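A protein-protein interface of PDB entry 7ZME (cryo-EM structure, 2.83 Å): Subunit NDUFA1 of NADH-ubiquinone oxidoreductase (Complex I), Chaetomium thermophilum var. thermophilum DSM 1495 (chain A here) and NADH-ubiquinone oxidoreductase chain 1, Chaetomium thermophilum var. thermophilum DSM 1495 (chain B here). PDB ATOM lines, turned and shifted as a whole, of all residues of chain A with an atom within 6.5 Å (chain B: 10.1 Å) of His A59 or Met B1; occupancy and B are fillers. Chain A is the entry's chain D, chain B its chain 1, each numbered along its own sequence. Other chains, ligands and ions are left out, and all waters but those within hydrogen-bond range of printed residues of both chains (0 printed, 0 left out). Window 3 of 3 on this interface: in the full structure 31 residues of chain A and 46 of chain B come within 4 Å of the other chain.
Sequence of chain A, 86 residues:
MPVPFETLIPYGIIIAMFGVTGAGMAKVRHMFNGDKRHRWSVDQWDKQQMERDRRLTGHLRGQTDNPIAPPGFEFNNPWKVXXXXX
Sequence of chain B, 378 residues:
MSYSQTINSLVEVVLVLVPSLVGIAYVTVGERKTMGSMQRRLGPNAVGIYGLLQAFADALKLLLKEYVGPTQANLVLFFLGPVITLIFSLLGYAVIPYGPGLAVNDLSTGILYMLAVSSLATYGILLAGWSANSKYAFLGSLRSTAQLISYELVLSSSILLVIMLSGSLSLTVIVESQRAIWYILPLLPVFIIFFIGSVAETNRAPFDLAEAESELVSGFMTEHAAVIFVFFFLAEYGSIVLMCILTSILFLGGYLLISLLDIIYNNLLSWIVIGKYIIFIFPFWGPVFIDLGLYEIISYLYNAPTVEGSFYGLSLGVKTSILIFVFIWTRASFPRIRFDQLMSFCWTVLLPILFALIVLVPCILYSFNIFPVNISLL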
ATOM      1  N   MET A  31     -18.441  30.456 -23.036  1.00  0.00           N
ATOM      2  CA  MET A  31     -17.935  29.336 -22.199  1.00  0.00           C
ATOM      3  C   MET A  31     -18.470  27.998 -22.676  1.00  0.00           C
ATOM      4  O   MET A  31     -17.663  27.078 -22.821  1.00  0.00           O
ATOM      5  CB  MET A  31     -18.395  29.508 -20.752  1.00  0.00           C
ATOM      6  CG  MET A  31     -17.814  30.740 -20.084  1.00  0.00           C
ATOM      7  SD  MET A  31     -16.011  30.821 -20.229  1.00  0.00           S
ATOM      8  CE  MET A  31     -15.823  32.137 -21.432  1.00  0.00           C
ATOM      9  N   PHE A  32     -19.765  27.912 -22.952  1.00  0.00           N
ATOM     10  CA  PHE A  32     -20.421  26.656 -23.375  1.00  0.00           C
ATOM     11  C   PHE A  32     -19.836  26.221 -24.720  1.00  0.00           C
ATOM     12  O   PHE A  32     -19.849  25.019 -25.023  1.00  0.00           O
ATOM     13  CB  PHE A  32     -21.914  26.948 -23.483  1.00  0.00           C
ATOM     14  CG  PHE A  32     -22.839  25.763 -23.502  1.00  0.00           C
ATOM     15  CD1 PHE A  32     -22.812  24.821 -22.489  1.00  0.00           C
ATOM     16  CD2 PHE A  32     -23.771  25.618 -24.516  1.00  0.00           C
ATOM     17  CE1 PHE A  32     -23.682  23.744 -22.507  1.00  0.00           C
ATOM     18  CE2 PHE A  32     -24.643  24.542 -24.529  1.00  0.00           C
ATOM     19  CZ  PHE A  32     -24.597  23.607 -23.524  1.00  0.00           C
ATOM     20  N   ASN A  33     -19.336  27.176 -25.497  1.00  0.00           N
ATOM     21  CA  ASN A  33     -18.819  26.895 -26.855  1.00  0.00           C
ATOM     22  C   ASN A  33     -17.295  26.881 -26.840  1.00  0.00           C
ATOM     23  O   ASN A  33     -16.716  27.212 -27.869  1.00  0.00           O
ATOM     24  CB  ASN A  33     -19.413  27.858 -27.879  1.00  0.00           C
ATOM     25  CG  ASN A  33     -20.852  27.550 -28.232  1.00  0.00           C
ATOM     26  OD1 ASN A  33     -21.121  26.916 -29.246  1.00  0.00           O
ATOM     27  ND2 ASN A  33     -21.786  27.997 -27.411  1.00  0.00           N
ATOM     28  N   GLY A  34     -16.677  26.479 -25.735  1.00  0.00           N
ATOM     29  CA  GLY A  34     -15.217  26.352 -25.665  1.00  0.00           C
ATOM     30  C   GLY A  34     -14.490  27.662 -25.839  1.00  0.00           C
ATOM     31  O   GLY A  34     -13.487  27.669 -26.581  1.00  0.00           O
ATOM     32  N   LYS A  36     -15.312  30.208 -27.483  1.00  0.00           N
ATOM     33  CA  LYS A  36     -15.359  30.583 -28.905  1.00  0.00           C
ATOM     34  C   LYS A  36     -16.666  31.322 -29.082  1.00  0.00           C
ATOM     35  O   LYS A  36     -17.559  31.090 -28.272  1.00  0.00           O
ATOM     36  CB  LYS A  36     -15.405  29.327 -29.774  1.00  0.00           C
ATOM     37  CG  LYS A  36     -14.113  28.533 -29.883  1.00  0.00           C
ATOM     38  CD  LYS A  36     -14.349  27.108 -30.334  1.00  0.00           C
ATOM     39  CE  LYS A  36     -13.082  26.386 -30.741  1.00  0.00           C
ATOM     40  NZ  LYS A  36     -12.626  26.796 -32.091  1.00  0.00           N
ATOM     41  N   MET A  50     -21.105  20.290 -37.256  1.00  0.00           N
ATOM     42  CA  MET A  50     -20.768  20.293 -35.811  1.00  0.00           C
ATOM     43  C   MET A  50     -20.713  18.856 -35.298  1.00  0.00           C
ATOM     44  O   MET A  50     -19.880  18.580 -34.429  1.00  0.00           O
ATOM     45  CB  MET A  50     -21.748  21.145 -34.999  1.00  0.00           C
ATOM     46  CG  MET A  50     -21.444  22.625 -35.109  1.00  0.00           C
ATOM     47  SD  MET A  50     -22.568  23.715 -34.213  1.00  0.00           S
ATOM     48  CE  MET A  50     -24.114  23.372 -35.051  1.00  0.00           C
ATOM     49  N   ASP A  53     -17.516  17.386 -36.349  1.00  0.00           N
ATOM     50  CA  ASP A  53     -16.424  17.911 -35.479  1.00  0.00           C
ATOM     51  C   ASP A  53     -16.322  17.116 -34.169  1.00  0.00           C
ATOM     52  O   ASP A  53     -15.198  16.884 -33.723  1.00  0.00           O
ATOM     53  CB  ASP A  53     -16.628  19.399 -35.182  1.00  0.00           C
ATOM     54  CG  ASP A  53     -16.396  20.306 -36.371  1.00  0.00           C
ATOM     55  OD1 ASP A  53     -15.943  19.804 -37.409  1.00  0.00           O
ATOM     56  OD2 ASP A  53     -16.675  21.508 -36.244  1.00  0.00           O
ATOM     57  N   ARG A  54     -17.452  16.752 -33.560  1.00  0.00           N
ATOM     58  CA  ARG A  54     -17.462  15.915 -32.332  1.00  0.00           C
ATOM     59  C   ARG A  54     -16.855  14.557 -32.682  1.00  0.00           C
ATOM     60  O   ARG A  54     -16.160  13.989 -31.839  1.00  0.00           O
ATOM     61  CB  ARG A  54     -18.883  15.817 -31.771  1.00  0.00           C
ATOM     62  CG  ARG A  54     -18.963  15.246 -30.365  1.00  0.00           C
ATOM     63  CD  ARG A  54     -20.201  14.422 -30.081  1.00  0.00           C
ATOM     64  NE  ARG A  54     -21.326  15.161 -29.526  1.00  0.00           N
ATOM     65  CZ  ARG A  54     -22.503  15.291 -30.120  1.00  0.00           C
ATOM     66  NH1 ARG A  54     -23.470  15.969 -29.527  1.00  0.00           N
ATOM     67  NH2 ARG A  54     -22.711  14.739 -31.300  1.00  0.00           N
ATOM     68  N   ARG A  55     -17.103  14.065 -33.895  1.00  0.00           N
ATOM     69  CA  ARG A  55     -16.525  12.783 -34.359  1.00  0.00           C
ATOM     70  C   ARG A  55     -14.991  12.849 -34.358  1.00  0.00           C
ATOM     71  O   ARG A  55     -14.373  11.806 -34.105  1.00  0.00           O
ATOM     72  CB  ARG A  55     -17.092  12.413 -35.728  1.00  0.00           C
ATOM     73  CG  ARG A  55     -18.532  11.932 -35.718  1.00  0.00           C
ATOM     74  CD  ARG A  55     -18.968  11.696 -37.147  1.00  0.00           C
ATOM     75  NE  ARG A  55     -18.202  10.631 -37.772  1.00  0.00           N
ATOM     76  CZ  ARG A  55     -18.164  10.405 -39.077  1.00  0.00           C
ATOM     77  NH1 ARG A  55     -18.837  11.186 -39.903  1.00  0.00           N
ATOM     78  NH2 ARG A  55     -17.444   9.406 -39.554  1.00  0.00           N
ATOM     79  N   LEU A  56     -14.396  14.002 -34.672  1.00  0.00           N
ATOM     80  CA  LEU A  56     -12.916  14.113 -34.755  1.00  0.00           C
ATOM     81  C   LEU A  56     -12.310  14.638 -33.445  1.00  0.00           C
ATOM     82  O   LEU A  56     -11.187  14.233 -33.142  1.00  0.00           O
ATOM     83  CB  LEU A  56     -12.574  15.055 -35.912  1.00  0.00           C
ATOM     84  CG  LEU A  56     -12.896  14.558 -37.319  1.00  0.00           C
ATOM     85  CD1 LEU A  56     -13.347  15.701 -38.212  1.00  0.00           C
ATOM     86  CD2 LEU A  56     -11.699  13.848 -37.928  1.00  0.00           C
ATOM     87  N   THR A  57     -13.009  15.484 -32.684  1.00  0.00           N
ATOM     88  CA  THR A  57     -12.417  16.090 -31.500  1.00  0.00           C
ATOM     89  C   THR A  57     -13.159  15.802 -30.206  1.00  0.00           C
ATOM     90  O   THR A  57     -12.582  16.007 -29.134  1.00  0.00           O
ATOM     91  CB  THR A  57     -12.319  17.619 -31.662  1.00  0.00           C
ATOM     92  OG1 THR A  57     -13.609  18.207 -31.462  1.00  0.00           O
ATOM     93  CG2 THR A  57     -11.796  17.996 -33.044  1.00  0.00           C
ATOM     94  N   GLY A  58     -14.408  15.347 -30.266  1.00  0.00           N
ATOM     95  CA  GLY A  58     -15.203  15.112 -29.084  1.00  0.00           C
ATOM     96  C   GLY A  58     -16.061  16.282 -28.659  1.00  0.00           C
ATOM     97  O   GLY A  58     -17.056  16.084 -27.956  1.00  0.00           O
ATOM     98  N   HIS A  59     -15.734  17.477 -29.147  1.00  0.00           N
ATOM     99  CA  HIS A  59     -16.535  18.689 -28.842  1.00  0.00           C
ATOM    100  C   HIS A  59     -17.185  19.149 -30.141  1.00  0.00           C
ATOM    101  O   HIS A  59     -16.483  19.171 -31.154  1.00  0.00           O
ATOM    102  CB  HIS A  59     -15.621  19.766 -28.252  1.00  0.00           C
ATOM    103  CG  HIS A  59     -16.320  20.885 -27.554  1.00  0.00           C
ATOM    104  ND1 HIS A  59     -16.769  22.007 -28.217  1.00  0.00           N
ATOM    105  CD2 HIS A  59     -16.609  21.080 -26.250  1.00  0.00           C
ATOM    106  CE1 HIS A  59     -17.325  22.835 -27.357  1.00  0.00           C
ATOM    107  NE2 HIS A  59     -17.234  22.291 -26.143  1.00  0.00           N
ATOM    108  N   LEU A  60     -18.486  19.466 -30.099  1.00  0.00           N
ATOM    109  CA  LEU A  60     -19.264  19.888 -31.298  1.00  0.00           C
ATOM    110  C   LEU A  60     -18.626  21.112 -31.943  1.00  0.00           C
ATOM    111  O   LEU A  60     -18.824  21.313 -33.137  1.00  0.00           O
ATOM    112  CB  LEU A  60     -20.703  20.196 -30.880  1.00  0.00           C
ATOM    113  CG  LEU A  60     -21.597  19.000 -30.576  1.00  0.00           C
ATOM    114  CD1 LEU A  60     -22.689  19.398 -29.596  1.00  0.00           C
ATOM    115  CD2 LEU A  60     -22.197  18.454 -31.858  1.00  0.00           C
ATOM    116  N   ARG A  61     -17.890  21.894 -31.164  1.00  0.00           N
ATOM    117  CA  ARG A  61     -17.263  23.136 -31.664  1.00  0.00           C
ATOM    118  C   ARG A  61     -15.759  22.951 -31.830  1.00  0.00           C
ATOM    119  O   ARG A  61     -15.084  23.962 -32.043  1.00  0.00           O
ATOM    120  CB  ARG A  61     -17.582  24.268 -30.687  1.00  0.00           C
ATOM    121  CG  ARG A  61     -19.047  24.676 -30.668  1.00  0.00           C
ATOM    122  CD  ARG A  61     -19.474  25.227 -32.012  1.00  0.00           C
ATOM    123  NE  ARG A  61     -18.507  26.167 -32.559  1.00  0.00           N
ATOM    124  CZ  ARG A  61     -18.462  27.461 -32.268  1.00  0.00           C
ATOM    125  NH1 ARG A  61     -17.546  28.234 -32.822  1.00  0.00           N
ATOM    126  NH2 ARG A  61     -19.332  27.980 -31.425  1.00  0.00           N
ATOM    127  N   GLY A  62     -15.256  21.720 -31.788  1.00  0.00           N
ATOM    128  CA  GLY A  62     -13.802  21.466 -31.857  1.00  0.00           C
ATOM    129  C   GLY A  62     -13.251  21.416 -33.266  1.00  0.00           C
ATOM    130  O   GLY A  62     -13.908  20.825 -34.119  1.00  0.00           O
ATOM    131  N   GLN A  63     -12.071  21.993 -33.497  1.00  0.00           N
ATOM    132  CA  GLN A  63     -11.520  22.073 -34.876  1.00  0.00           C
ATOM    133  C   GLN A  63     -10.136  21.428 -34.999  1.00  0.00           C
ATOM    134  O   GLN A  63      -9.291  21.692 -34.151  1.00  0.00           O
ATOM    135  CB  GLN A  63     -11.565  23.504 -35.421  1.00  0.00           C
ATOM    136  CG  GLN A  63     -12.868  24.249 -35.168  1.00  0.00           C
ATOM    137  CD  GLN A  63     -14.034  23.766 -35.993  1.00  0.00           C
ATOM    138  OE1 GLN A  63     -13.880  23.272 -37.105  1.00  0.00           O
ATOM    139  NE2 GLN A  63     -15.230  23.923 -35.452  1.00  0.00           N
ATOM    140  N   MET B   1     -20.494  19.961 -25.972  1.00  0.00           N
ATOM    141  CA  MET B   1     -20.348  21.314 -25.377  1.00  0.00           C
ATOM    142  C   MET B   1     -19.446  21.248 -24.143  1.00  0.00           C
ATOM    143  O   MET B   1     -18.811  20.199 -23.960  1.00  0.00           O
ATOM    144  CB  MET B   1     -21.695  21.972 -25.090  1.00  0.00           C
ATOM    145  CG  MET B   1     -22.453  22.329 -26.354  1.00  0.00           C
ATOM    146  SD  MET B   1     -21.420  23.186 -27.571  1.00  0.00           S
ATOM    147  CE  MET B   1     -22.654  23.665 -28.777  1.00  0.00           C
ATOM    148  N   SER B   2     -19.401  22.297 -23.318  1.00  0.00           N
ATOM    149  CA  SER B   2     -18.391  22.330 -22.227  1.00  0.00           C
ATOM    150  C   SER B   2     -18.995  21.912 -20.892  1.00  0.00           C
ATOM    151  O   SER B   2     -18.518  20.910 -20.328  1.00  0.00           O
ATOM    152  CB  SER B   2     -17.784  23.703 -22.132  1.00  0.00           C
ATOM    153  OG  SER B   2     -17.235  24.106 -23.378  1.00  0.00           O
ATOM    154  N   TYR B   3     -19.981  22.657 -20.396  1.00  0.00           N
ATOM    155  CA  TYR B   3     -20.645  22.247 -19.168  1.00  0.00           C
ATOM    156  C   TYR B   3     -22.048  21.742 -19.499  1.00  0.00           C
ATOM    157  O   TYR B   3     -22.396  21.537 -20.664  1.00  0.00           O
ATOM    158  CB  TYR B   3     -20.657  23.388 -18.148  1.00  0.00           C
ATOM    159  CG  TYR B   3     -21.240  24.691 -18.644  1.00  0.00           C
ATOM    160  CD1 TYR B   3     -20.444  25.638 -19.268  1.00  0.00           C
ATOM    161  CD2 TYR B   3     -22.583  24.984 -18.466  1.00  0.00           C
ATOM    162  CE1 TYR B   3     -20.971  26.828 -19.711  1.00  0.00           C
ATOM    163  CE2 TYR B   3     -23.118  26.172 -18.907  1.00  0.00           C
ATOM    164  CZ  TYR B   3     -22.308  27.090 -19.530  1.00  0.00           C
ATOM    165  OH  TYR B   3     -22.839  28.279 -19.971  1.00  0.00           O
ATOM    166  N   SER B   4     -22.841  21.515 -18.456  1.00  0.00           N
ATOM    167  CA  SER B   4     -24.147  20.889 -18.613  1.00  0.00           C
ATOM    168  C   SER B   4     -25.074  21.742 -19.470  1.00  0.00           C
ATOM    169  O   SER B   4     -25.030  22.973 -19.443  1.00  0.00           O
ATOM    170  CB  SER B   4     -24.783  20.648 -17.245  1.00  0.00           C
ATOM    171  OG  SER B   4     -26.167  20.383 -17.367  1.00  0.00           O
ATOM    172  N   GLN B   5     -25.923  21.063 -20.244  1.00  0.00           N
ATOM    173  CA  GLN B   5     -26.890  21.758 -21.084  1.00  0.00           C
ATOM    174  C   GLN B   5     -27.999  22.385 -20.251  1.00  0.00           C
ATOM    175  O   GLN B   5     -28.425  23.513 -20.523  1.00  0.00           O
ATOM    176  CB  GLN B   5     -27.473  20.793 -22.115  1.00  0.00           C
ATOM    177  CG  GLN B   5     -28.671  21.328 -22.873  1.00  0.00           C
ATOM    178  CD  GLN B   5     -28.279  22.103 -24.114  1.00  0.00           C
ATOM    179  OE1 GLN B   5     -27.580  21.588 -24.987  1.00  0.00           O
ATOM    180  NE2 GLN B   5     -28.733  23.347 -24.203  1.00  0.00           N
ATOM    181  N   THR B   6     -28.484  21.669 -19.236  1.00  0.00           N
ATOM    182  CA  THR B   6     -29.563  22.199 -18.410  1.00  0.00           C
ATOM    183  C   THR B   6     -29.111  23.425 -17.627  1.00  0.00           C
ATOM    184  O   THR B   6     -29.877  24.381 -17.461  1.00  0.00           O
ATOM    185  CB  THR B   6     -30.079  21.116 -17.464  1.00  0.00           C
ATOM    186  OG1 THR B   6     -30.574  20.011 -18.230  1.00  0.00           O
ATOM    187  CG2 THR B   6     -31.203  21.653 -16.597  1.00  0.00           C
ATOM    188  N   ASN B   8     -26.775  25.525 -18.584  1.00  0.00           N
ATOM    189  CA  ASN B   8     -26.676  26.618 -19.543  1.00  0.00           C
ATOM    190  C   ASN B   8     -28.033  27.266 -19.764  1.00  0.00           C
ATOM    191  O   ASN B   8     -28.184  28.483 -19.622  1.00  0.00           O
ATOM    192  CB  ASN B   8     -26.103  26.111 -20.866  1.00  0.00           C
ATOM    193  CG  ASN B   8     -25.950  27.213 -21.894  1.00  0.00           C
ATOM    194  OD1 ASN B   8     -26.658  27.246 -22.899  1.00  0.00           O
ATOM    195  ND2 ASN B   8     -25.020  28.124 -21.647  1.00  0.00           N
ATOM    196  N   SER B   9     -29.044  26.455 -20.075  1.00  0.00           N
ATOM    197  CA  SER B   9     -30.384  26.976 -20.316  1.00  0.00           C
ATOM    198  C   SER B   9     -30.964  27.623 -19.069  1.00  0.00           C
ATOM    199  O   SER B   9     -31.718  28.597 -19.167  1.00  0.00           O
ATOM    200  CB  SER B   9     -31.289  25.848 -20.799  1.00  0.00           C
ATOM    201  OG  SER B   9     -30.665  25.119 -21.839  1.00  0.00           O
ATOM    202  N   GLU B  12     -29.208  31.037 -18.927  1.00  0.00           N
ATOM    203  CA  GLU B  12     -29.623  31.837 -20.101  1.00  0.00           C
ATOM    204  C   GLU B  12     -31.025  32.405 -19.912  1.00  0.00           C
ATOM    205  O   GLU B  12     -31.269  33.526 -20.350  1.00  0.00           O
ATOM    206  CB  GLU B  12     -29.406  31.056 -21.391  1.00  0.00           C
ATOM    207  CG  GLU B  12     -27.944  30.959 -21.765  1.00  0.00           C
ATOM    208  CD  GLU B  12     -27.683  30.676 -23.230  1.00  0.00           C
ATOM    209  OE1 GLU B  12     -28.661  30.499 -23.981  1.00  0.00           O
ATOM    210  OE2 GLU B  12     -26.501  30.639 -23.614  1.00  0.00           O
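Among the printed residues, merely in contact across the chains: Met A31 with Tyr B3 (3.9 Å), Phe A32 with Tyr B3 (3.1 Å), Phe A32 with Ser B4 (3.4 Å), Phe A32 with Gln B5 (3.8 Å), Phe A32 with Asn B8 (3.7 Å) and Asn A33 with Met B1 (3.6 Å).
Hydrophobic or aromatic side chains of chain B that line the printed part of chain A: Met B1 and Tyr B3. Of the 17 printed residues of chain A, 5 touch a printed residue of chain B. Printed residues of chain A that touch a printed residue of chain B: Met A31, Phe A32, Asn A33, Gly A34 and His A59. Hydrophobic or aromatic side chains of chain A that line the printed part of chain B: Met A31, Phe A32 and His A59. Among the printed residues, no Asp or Glu carboxylate lies within 4 Å of a Lys or Arg side-chain nitrogen of the other chain.
A ring nitrogen (ND1) of His A59 sits close to the backbone NH (N) of Arg A61 (3.2 Å). The side-chain hydroxyl (OG1) of Thr A57 sits at hydrogen-bond distance from the backbone carbonyl oxygen (O) of His A59 (3.0 Å). The side-chain amide nitrogen (ND2) of Asn B8 is in hydrogen-bond range of the side-chain hydroxyl (OH) of Tyr B3 (2.8 Å). The side-chain amide oxygen (OD1) of Asn A33 is in hydrogen-bond range of the guanidinium group (NH2) of Arg A61, 3.0 Å away. O of Gln B5 lies within hydrogen-bond range of OG of Ser B9. The backbone NH (N) of Thr B6 lies within hydrogen-bond range of the side-chain hydroxyl (OG) of Ser B4 (3.2 Å).
NE2 of His A59 lies close to O of Met B1, at 3.4 Å. A ring nitrogen (NE2) of His A59 sits at hydrogen-bond distance from the side-chain hydroxyl (OG) of Ser B2 (3.3 Å). OG of Ser B2 is in hydrogen-bond range of O of Phe A32, 3.2 Å away. The backbone carbonyl oxygen of Phe A32 sits close to the side-chain sulfur of Met B1, at 3.5 Å. The side-chain hydroxyl (OG) of Ser B2 sits at hydrogen-bond distance from the backbone carbonyl oxygen (O) of Met A31 (3.1 Å). The backbone NH (N) of Gly A34 sits at hydrogen-bond distance from the side-chain hydroxyl (OG) of Ser B2, at 3.4 Å.
Of chain B, only Met B1 (3.2 Å) and Ser B2 (3.3 Å) come within 4 Å of His A59. Met B1 touches just these residues of chain A: Phe A32 (3.5 Å), Asn A33 (3.6 Å) and His A59 (3.2 Å). No residue of chain B comes within 4 Å of Thr A57. No residue of chain B comes within 4 Å of Gly A58. No residue of chain B comes within 4 Å of Gly A62. Of the printed residues of chain A, Gln B5 touches Phe A32. Printed residues of chain A within 4 Å of Tyr B3: Met A31 (3.9 Å) and Phe A32 (3.1 Å). Met A50 touches none of the printed residues of chain B. The nearest printed residue of chain A that does not touch Ser B4 is Met A31 (8.8 Å).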
